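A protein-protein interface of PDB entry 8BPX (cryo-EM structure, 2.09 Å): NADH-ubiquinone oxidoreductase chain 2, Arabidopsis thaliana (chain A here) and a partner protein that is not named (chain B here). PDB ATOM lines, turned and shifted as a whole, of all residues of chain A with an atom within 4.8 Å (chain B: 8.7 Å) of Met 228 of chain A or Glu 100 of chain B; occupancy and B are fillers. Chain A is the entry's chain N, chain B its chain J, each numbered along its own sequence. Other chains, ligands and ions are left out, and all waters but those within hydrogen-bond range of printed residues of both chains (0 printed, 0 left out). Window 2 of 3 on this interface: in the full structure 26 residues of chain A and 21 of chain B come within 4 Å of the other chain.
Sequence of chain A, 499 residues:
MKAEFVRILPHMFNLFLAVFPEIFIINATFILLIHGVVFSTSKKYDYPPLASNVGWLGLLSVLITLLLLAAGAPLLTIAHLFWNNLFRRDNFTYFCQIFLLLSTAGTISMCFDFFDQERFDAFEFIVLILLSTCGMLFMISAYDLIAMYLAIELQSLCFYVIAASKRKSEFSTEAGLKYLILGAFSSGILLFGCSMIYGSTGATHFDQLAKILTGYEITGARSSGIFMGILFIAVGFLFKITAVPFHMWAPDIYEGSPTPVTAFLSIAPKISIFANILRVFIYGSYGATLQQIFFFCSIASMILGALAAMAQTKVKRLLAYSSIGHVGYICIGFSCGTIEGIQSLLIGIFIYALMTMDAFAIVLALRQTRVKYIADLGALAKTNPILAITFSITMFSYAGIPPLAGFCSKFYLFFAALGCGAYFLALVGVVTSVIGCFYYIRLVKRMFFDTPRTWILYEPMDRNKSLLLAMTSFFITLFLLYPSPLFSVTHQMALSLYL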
ATOM      1  N   GLY A 193      -5.100  -9.294  16.389  1.00  0.00           N
ATOM      2  CA  GLY A 193      -4.019  -9.653  17.296  1.00  0.00           C
ATOM      3  C   GLY A 193      -2.979 -10.542  16.638  1.00  0.00           C
ATOM      4  O   GLY A 193      -1.771 -10.347  16.817  1.00  0.00           O
ATOM      5  N   SER A 224       5.334  -3.233  21.990  1.00  0.00           N
ATOM      6  CA  SER A 224       3.916  -2.929  22.109  1.00  0.00           C
ATOM      7  C   SER A 224       3.094  -3.702  21.081  1.00  0.00           C
ATOM      8  O   SER A 224       1.932  -4.041  21.339  1.00  0.00           O
ATOM      9  CB  SER A 224       3.717  -1.418  21.986  1.00  0.00           C
ATOM     10  OG  SER A 224       3.395  -1.037  20.670  1.00  0.00           O
ATOM     11  N   GLY A 225       3.696  -4.025  19.934  1.00  0.00           N
ATOM     12  CA  GLY A 225       3.010  -4.850  18.952  1.00  0.00           C
ATOM     13  C   GLY A 225       2.694  -6.241  19.466  1.00  0.00           C
ATOM     14  O   GLY A 225       1.559  -6.710  19.360  1.00  0.00           O
ATOM     15  N   ILE A 226       3.710  -6.863  20.065  1.00  0.00           N
ATOM     16  CA  ILE A 226       3.550  -8.173  20.748  1.00  0.00           C
ATOM     17  C   ILE A 226       2.552  -8.063  21.906  1.00  0.00           C
ATOM     18  O   ILE A 226       1.652  -8.902  21.951  1.00  0.00           O
ATOM     19  CB  ILE A 226       4.896  -8.722  21.230  1.00  0.00           C
ATOM     20  CG1 ILE A 226       5.865  -8.978  20.077  1.00  0.00           C
ATOM     21  CG2 ILE A 226       4.701  -9.980  22.066  1.00  0.00           C
ATOM     22  CD1 ILE A 226       7.255  -9.344  20.537  1.00  0.00           C
ATOM     23  N   PHE A 227       2.633  -7.018  22.712  1.00  0.00           N
ATOM     24  CA  PHE A 227       1.733  -6.898  23.875  1.00  0.00           C
ATOM     25  C   PHE A 227       0.258  -6.759  23.411  1.00  0.00           C
ATOM     26  O   PHE A 227      -0.569  -7.446  23.982  1.00  0.00           O
ATOM     27  CB  PHE A 227       2.205  -5.782  24.808  1.00  0.00           C
ATOM     28  CG  PHE A 227       1.456  -5.684  26.094  1.00  0.00           C
ATOM     29  CD1 PHE A 227       0.249  -5.015  26.150  1.00  0.00           C
ATOM     30  CD2 PHE A 227       1.953  -6.291  27.232  1.00  0.00           C
ATOM     31  CE1 PHE A 227      -0.440  -4.932  27.343  1.00  0.00           C
ATOM     32  CE2 PHE A 227       1.262  -6.200  28.420  1.00  0.00           C
ATOM     33  CZ  PHE A 227       0.067  -5.527  28.470  1.00  0.00           C
ATOM     34  N   MET A 228      -0.037  -5.959  22.399  1.00  0.00           N
ATOM     35  CA  MET A 228      -1.420  -5.788  21.962  1.00  0.00           C
ATOM     36  C   MET A 228      -1.910  -6.943  21.102  1.00  0.00           C
ATOM     37  O   MET A 228      -3.107  -7.255  21.114  1.00  0.00           O
ATOM     38  CB  MET A 228      -1.592  -4.447  21.261  1.00  0.00           C
ATOM     39  CG  MET A 228      -1.125  -3.362  22.163  1.00  0.00           C
ATOM     40  SD  MET A 228      -2.592  -2.509  22.737  1.00  0.00           S
ATOM     41  CE  MET A 228      -1.853  -1.491  23.988  1.00  0.00           C
ATOM     42  N   GLY A 229      -1.020  -7.604  20.360  1.00  0.00           N
ATOM     43  CA  GLY A 229      -1.430  -8.825  19.685  1.00  0.00           C
ATOM     44  C   GLY A 229      -1.914  -9.869  20.671  1.00  0.00           C
ATOM     45  O   GLY A 229      -2.971 -10.484  20.485  1.00  0.00           O
ATOM     46  N   ILE A 230      -1.136 -10.084  21.725  1.00  0.00           N
ATOM     47  CA  ILE A 230      -1.562 -10.982  22.837  1.00  0.00           C
ATOM     48  C   ILE A 230      -2.914 -10.506  23.395  1.00  0.00           C
ATOM     49  O   ILE A 230      -3.748 -11.305  23.601  1.00  0.00           O
ATOM     50  CB  ILE A 230      -0.496 -11.076  23.978  1.00  0.00           C
ATOM     51  CG1 ILE A 230       0.839 -11.601  23.461  1.00  0.00           C
ATOM     52  CG2 ILE A 230      -1.001 -11.872  25.165  1.00  0.00           C
ATOM     53  CD1 ILE A 230       0.705 -12.888  22.739  1.00  0.00           C
ATOM     54  N   LEU A 231      -3.070  -9.236  23.657  1.00  0.00           N
ATOM     55  CA  LEU A 231      -4.321  -8.771  24.252  1.00  0.00           C
ATOM     56  C   LEU A 231      -5.518  -9.079  23.358  1.00  0.00           C
ATOM     57  O   LEU A 231      -6.550  -9.571  23.831  1.00  0.00           O
ATOM     58  CB  LEU A 231      -4.256  -7.275  24.534  1.00  0.00           C
ATOM     59  CG  LEU A 231      -3.647  -6.927  25.883  1.00  0.00           C
ATOM     60  CD1 LEU A 231      -3.411  -5.430  25.966  1.00  0.00           C
ATOM     61  CD2 LEU A 231      -4.521  -7.445  27.005  1.00  0.00           C
ATOM     62  N   PHE A 232      -5.402  -8.785  22.061  1.00  0.00           N
ATOM     63  CA  PHE A 232      -6.520  -9.014  21.149  1.00  0.00           C
ATOM     64  C   PHE A 232      -6.832 -10.504  21.019  1.00  0.00           C
ATOM     65  O   PHE A 232      -8.008 -10.906  20.995  1.00  0.00           O
ATOM     66  CB  PHE A 232      -6.214  -8.392  19.784  1.00  0.00           C
ATOM     67  CG  PHE A 232      -6.506  -6.910  19.705  1.00  0.00           C
ATOM     68  CD1 PHE A 232      -5.930  -6.022  20.600  1.00  0.00           C
ATOM     69  CD2 PHE A 232      -7.354  -6.409  18.733  1.00  0.00           C
ATOM     70  CE1 PHE A 232      -6.192  -4.665  20.528  1.00  0.00           C
ATOM     71  CE2 PHE A 232      -7.622  -5.049  18.656  1.00  0.00           C
ATOM     72  CZ  PHE A 232      -7.039  -4.178  19.555  1.00  0.00           C
ATOM     73  N   ILE B  92     -13.753   9.478  22.800  1.00  0.00           N
ATOM     74  CA  ILE B  92     -12.828   8.720  23.696  1.00  0.00           C
ATOM     75  C   ILE B  92     -12.385   7.446  22.959  1.00  0.00           C
ATOM     76  O   ILE B  92     -11.174   7.294  22.732  1.00  0.00           O
ATOM     77  CB  ILE B  92     -13.439   8.450  25.089  1.00  0.00           C
ATOM     78  CG1 ILE B  92     -14.127   9.699  25.644  1.00  0.00           C
ATOM     79  CG2 ILE B  92     -12.394   7.921  26.053  1.00  0.00           C
ATOM     80  CD1 ILE B  92     -15.507   9.450  26.194  1.00  0.00           C
ATOM     81  N   ILE B  93     -13.322   6.588  22.563  1.00  0.00           N
ATOM     82  CA  ILE B  93     -12.921   5.291  22.024  1.00  0.00           C
ATOM     83  C   ILE B  93     -12.005   5.480  20.823  1.00  0.00           C
ATOM     84  O   ILE B  93     -10.985   4.796  20.687  1.00  0.00           O
ATOM     85  CB  ILE B  93     -14.157   4.444  21.669  1.00  0.00           C
ATOM     86  CG1 ILE B  93     -14.992   4.153  22.919  1.00  0.00           C
ATOM     87  CG2 ILE B  93     -13.730   3.140  21.031  1.00  0.00           C
ATOM     88  CD1 ILE B  93     -14.370   3.165  23.863  1.00  0.00           C
ATOM     89  N   GLY B  94     -12.346   6.421  19.942  1.00  0.00           N
ATOM     90  CA  GLY B  94     -11.488   6.693  18.802  1.00  0.00           C
ATOM     91  C   GLY B  94     -10.119   7.201  19.211  1.00  0.00           C
ATOM     92  O   GLY B  94      -9.096   6.716  18.726  1.00  0.00           O
ATOM     93  N   LEU B  95     -10.103   8.227  20.075  1.00  0.00           N
ATOM     94  CA  LEU B  95      -8.820   8.811  20.560  1.00  0.00           C
ATOM     95  C   LEU B  95      -7.939   7.713  21.170  1.00  0.00           C
ATOM     96  O   LEU B  95      -6.797   7.592  20.740  1.00  0.00           O
ATOM     97  CB  LEU B  95      -9.071   9.916  21.586  1.00  0.00           C
ATOM     98  CG  LEU B  95      -7.824  10.556  22.192  1.00  0.00           C
ATOM     99  CD1 LEU B  95      -7.482  11.853  21.476  1.00  0.00           C
ATOM    100  CD2 LEU B  95      -8.011  10.800  23.682  1.00  0.00           C
ATOM    101  N   ILE B  96      -8.438   6.972  22.158  1.00  0.00           N
ATOM    102  CA  ILE B  96      -7.647   5.928  22.807  1.00  0.00           C
ATOM    103  C   ILE B  96      -7.093   4.964  21.771  1.00  0.00           C
ATOM    104  O   ILE B  96      -5.897   4.649  21.762  1.00  0.00           O
ATOM    105  CB  ILE B  96      -8.485   5.187  23.863  1.00  0.00           C
ATOM    106  CG1 ILE B  96      -8.949   6.144  24.964  1.00  0.00           C
ATOM    107  CG2 ILE B  96      -7.712   4.004  24.423  1.00  0.00           C
ATOM    108  CD1 ILE B  96      -9.792   5.478  26.025  1.00  0.00           C
ATOM    109  N   PHE B  97      -7.958   4.486  20.878  1.00  0.00           N
ATOM    110  CA  PHE B  97      -7.488   3.660  19.777  1.00  0.00           C
ATOM    111  C   PHE B  97      -6.518   4.436  18.897  1.00  0.00           C
ATOM    112  O   PHE B  97      -5.497   3.899  18.465  1.00  0.00           O
ATOM    113  CB  PHE B  97      -8.674   3.150  18.959  1.00  0.00           C
ATOM    114  CG  PHE B  97      -9.226   1.839  19.444  1.00  0.00           C
ATOM    115  CD1 PHE B  97     -10.209   1.808  20.419  1.00  0.00           C
ATOM    116  CD2 PHE B  97      -8.773   0.640  18.921  1.00  0.00           C
ATOM    117  CE1 PHE B  97     -10.729   0.608  20.868  1.00  0.00           C
ATOM    118  CE2 PHE B  97      -9.288  -0.568  19.367  1.00  0.00           C
ATOM    119  CZ  PHE B  97     -10.268  -0.580  20.344  1.00  0.00           C
ATOM    120  N   TRP B  98      -6.806   5.714  18.643  1.00  0.00           N
ATOM    121  CA  TRP B  98      -5.890   6.511  17.832  1.00  0.00           C
ATOM    122  C   TRP B  98      -4.521   6.636  18.494  1.00  0.00           C
ATOM    123  O   TRP B  98      -3.495   6.364  17.863  1.00  0.00           O
ATOM    124  CB  TRP B  98      -6.473   7.894  17.577  1.00  0.00           C
ATOM    125  CG  TRP B  98      -5.557   8.772  16.795  1.00  0.00           C
ATOM    126  CD1 TRP B  98      -5.305   8.715  15.456  1.00  0.00           C
ATOM    127  CD2 TRP B  98      -4.739   9.824  17.315  1.00  0.00           C
ATOM    128  NE1 TRP B  98      -4.394   9.680  15.107  1.00  0.00           N
ATOM    129  CE2 TRP B  98      -4.029  10.373  16.231  1.00  0.00           C
ATOM    130  CE3 TRP B  98      -4.542  10.357  18.591  1.00  0.00           C
ATOM    131  CZ2 TRP B  98      -3.138  11.430  16.383  1.00  0.00           C
ATOM    132  CZ3 TRP B  98      -3.656  11.407  18.741  1.00  0.00           C
ATOM    133  CH2 TRP B  98      -2.966  11.932  17.642  1.00  0.00           C
ATOM    134  N   TRP B  99      -4.492   7.034  19.768  1.00  0.00           N
ATOM    135  CA  TRP B  99      -3.223   7.273  20.453  1.00  0.00           C
ATOM    136  C   TRP B  99      -2.410   5.998  20.610  1.00  0.00           C
ATOM    137  O   TRP B  99      -1.176   6.033  20.584  1.00  0.00           O
ATOM    138  CB  TRP B  99      -3.481   7.900  21.822  1.00  0.00           C
ATOM    139  CG  TRP B  99      -2.260   7.946  22.690  1.00  0.00           C
ATOM    140  CD1 TRP B  99      -2.096   7.330  23.893  1.00  0.00           C
ATOM    141  CD2 TRP B  99      -1.023   8.624  22.416  1.00  0.00           C
ATOM    142  NE1 TRP B  99      -0.845   7.587  24.394  1.00  0.00           N
ATOM    143  CE2 TRP B  99      -0.166   8.378  23.506  1.00  0.00           C
ATOM    144  CE3 TRP B  99      -0.562   9.417  21.361  1.00  0.00           C
ATOM    145  CZ2 TRP B  99       1.126   8.895  23.572  1.00  0.00           C
ATOM    146  CZ3 TRP B  99       0.721   9.930  21.428  1.00  0.00           C
ATOM    147  CH2 TRP B  99       1.550   9.667  22.525  1.00  0.00           C
ATOM    148  N   GLU B 100      -3.077   4.867  20.767  1.00  0.00           N
ATOM    149  CA  GLU B 100      -2.368   3.619  20.982  1.00  0.00           C
ATOM    150  C   GLU B 100      -1.965   2.939  19.688  1.00  0.00           C
ATOM    151  O   GLU B 100      -0.871   2.378  19.597  1.00  0.00           O
ATOM    152  CB  GLU B 100      -3.259   2.654  21.755  1.00  0.00           C
ATOM    153  CG  GLU B 100      -2.542   1.420  22.151  1.00  0.00           C
ATOM    154  CD  GLU B 100      -1.714   1.658  23.367  1.00  0.00           C
ATOM    155  OE1 GLU B 100      -2.243   2.258  24.320  1.00  0.00           O
ATOM    156  OE2 GLU B 100      -0.525   1.281  23.350  1.00  0.00           O
ATOM    157  N   MET B 101      -2.818   2.992  18.699  1.00  0.00           N
ATOM    158  CA  MET B 101      -2.857   1.976  17.671  1.00  0.00           C
ATOM    159  C   MET B 101      -2.391   2.483  16.310  1.00  0.00           C
ATOM    160  O   MET B 101      -1.992   1.677  15.468  1.00  0.00           O
ATOM    161  CB  MET B 101      -4.284   1.404  17.629  1.00  0.00           C
ATOM    162  CG  MET B 101      -4.724   0.794  16.392  1.00  0.00           C
ATOM    163  SD  MET B 101      -4.697  -0.995  16.622  1.00  0.00           S
ATOM    164  CE  MET B 101      -6.032  -1.291  17.792  1.00  0.00           C
ATOM    165  N   PHE B 102      -2.426   3.796  16.074  1.00  0.00           N
ATOM    166  CA  PHE B 102      -1.738   4.388  14.927  1.00  0.00           C
ATOM    167  C   PHE B 102      -0.237   4.515  15.148  1.00  0.00           C
ATOM    168  O   PHE B 102       0.504   4.679  14.177  1.00  0.00           O
ATOM    169  CB  PHE B 102      -2.303   5.774  14.606  1.00  0.00           C
ATOM    170  CG  PHE B 102      -3.663   5.754  13.990  1.00  0.00           C
ATOM    171  CD1 PHE B 102      -4.769   5.387  14.739  1.00  0.00           C
ATOM    172  CD2 PHE B 102      -3.849   6.125  12.671  1.00  0.00           C
ATOM    173  CE1 PHE B 102      -6.024   5.373  14.172  1.00  0.00           C
ATOM    174  CE2 PHE B 102      -5.102   6.117  12.104  1.00  0.00           C
ATOM    175  CZ  PHE B 102      -6.188   5.741  12.854  1.00  0.00           C
ATOM    176  N   PHE B 103       0.220   4.443  16.401  1.00  0.00           N
ATOM    177  CA  PHE B 103       1.619   4.673  16.748  1.00  0.00           C
ATOM    178  C   PHE B 103       2.280   3.444  17.352  1.00  0.00           C
ATOM    179  O   PHE B 103       3.365   3.559  17.931  1.00  0.00           O
ATOM    180  CB  PHE B 103       1.731   5.857  17.717  1.00  0.00           C
ATOM    181  CG  PHE B 103       1.000   7.086  17.253  1.00  0.00           C
ATOM    182  CD1 PHE B 103       1.489   7.842  16.200  1.00  0.00           C
ATOM    183  CD2 PHE B 103      -0.187   7.471  17.854  1.00  0.00           C
ATOM    184  CE1 PHE B 103       0.815   8.968  15.763  1.00  0.00           C
ATOM    185  CE2 PHE B 103      -0.865   8.594  17.420  1.00  0.00           C
ATOM    186  CZ  PHE B 103      -0.364   9.343  16.372  1.00  0.00           C
ATOM    187  N   ILE B 104       1.653   2.272  17.232  1.00  0.00           N
ATOM    188  CA  ILE B 104       2.175   1.058  17.852  1.00  0.00           C
ATOM    189  C   ILE B 104       3.499   0.643  17.221  1.00  0.00           C
ATOM    190  O   ILE B 104       4.379   0.110  17.905  1.00  0.00           O
ATOM    191  CB  ILE B 104       1.112  -0.056  17.768  1.00  0.00           C
ATOM    192  CG1 ILE B 104       1.646  -1.392  18.277  1.00  0.00           C
ATOM    193  CG2 ILE B 104       0.612  -0.202  16.367  1.00  0.00           C
ATOM    194  CD1 ILE B 104       0.583  -2.262  18.892  1.00  0.00           C
ATOM    195  N   LEU B 105       3.667   0.886  15.921  1.00  0.00           N
ATOM    196  CA  LEU B 105       4.894   0.521  15.226  1.00  0.00           C
ATOM    197  C   LEU B 105       6.036   1.503  15.464  1.00  0.00           C
ATOM    198  O   LEU B 105       7.179   1.184  15.120  1.00  0.00           O
ATOM    199  CB  LEU B 105       4.639   0.413  13.717  1.00  0.00           C
ATOM    200  CG  LEU B 105       3.576  -0.553  13.192  1.00  0.00           C
ATOM    201  CD1 LEU B 105       3.792  -0.828  11.711  1.00  0.00           C
ATOM    202  CD2 LEU B 105       3.575  -1.851  13.972  1.00  0.00           C
ATOM    203  N   ASP B 106       5.762   2.676  16.040  1.00  0.00           N
ATOM    204  CA  ASP B 106       6.767   3.736  16.084  1.00  0.00           C
ATOM    205  C   ASP B 106       7.985   3.338  16.911  1.00  0.00           C
ATOM    206  O   ASP B 106       9.120   3.645  16.533  1.00  0.00           O
ATOM    207  CB  ASP B 106       6.143   5.024  16.618  1.00  0.00           C
ATOM    208  CG  ASP B 106       5.134   5.619  15.653  1.00  0.00           C
ATOM    209  OD1 ASP B 106       4.438   4.841  14.969  1.00  0.00           O
ATOM    210  OD2 ASP B 106       5.041   6.860  15.573  1.00  0.00           O
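Of the printed residues of chain B, Ser 224 of chain A touches Ile 104. Of the printed residues of chain B, Gly 225 of chain A touches Ile 104. Met 228 of chain A touches just these residues of chain B: Glu 100 and Ile 104. No residue of chain B comes within 4 Å of Gly 229 of chain A. Of the printed residues of chain B, Phe 232 of chain A touches Met 101. Glu 100 of chain B touches just one residue of chain A: Met 228 (3.1 Å). Printed residues of chain A within 4 Å of Met 101 of chain B: Phe 232. Of the printed residues of chain A, Ile 104 of chain B touches Ser 224, Gly 225 and Met 228. The nearest residue of chain B that does not touch Met 228 of chain A is Met 101 of chain B (6.1 Å). The nearest printed residue of chain A that does not touch Ile 104 of chain B is Ile 226 of chain A (5.7 Å).
OG of Ser 224 of chain A sits close to O of Ile 104 of chain B (3.2 Å).
Gly 225 of chain A touches Ile 104 of chain B. Met 228 of chain A touches Glu 100 of chain B (CE to OE2, 3.1 Å). CD1 of Ile 104 of chain B touches CG of Met 228 of chain A (3.9 Å). Phe 232 of chain A touches Met 101 of chain B.
Printed residues of chain B that touch a printed residue of chain A: Glu 100, Met 101 and Ile 104. Hydrophobic or aromatic side chains of chain B within 4 Å of the printed part of chain A: Met 101 and Ile 104. Hydrophobic or aromatic side chains of chain A within 4 Å of the printed part of chain B: Met 228 and Phe 232. Among the printed residues, no Asp or Glu carboxylate lies within 4 Å of a Lys or Arg side-chain nitrogen of the other chain.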
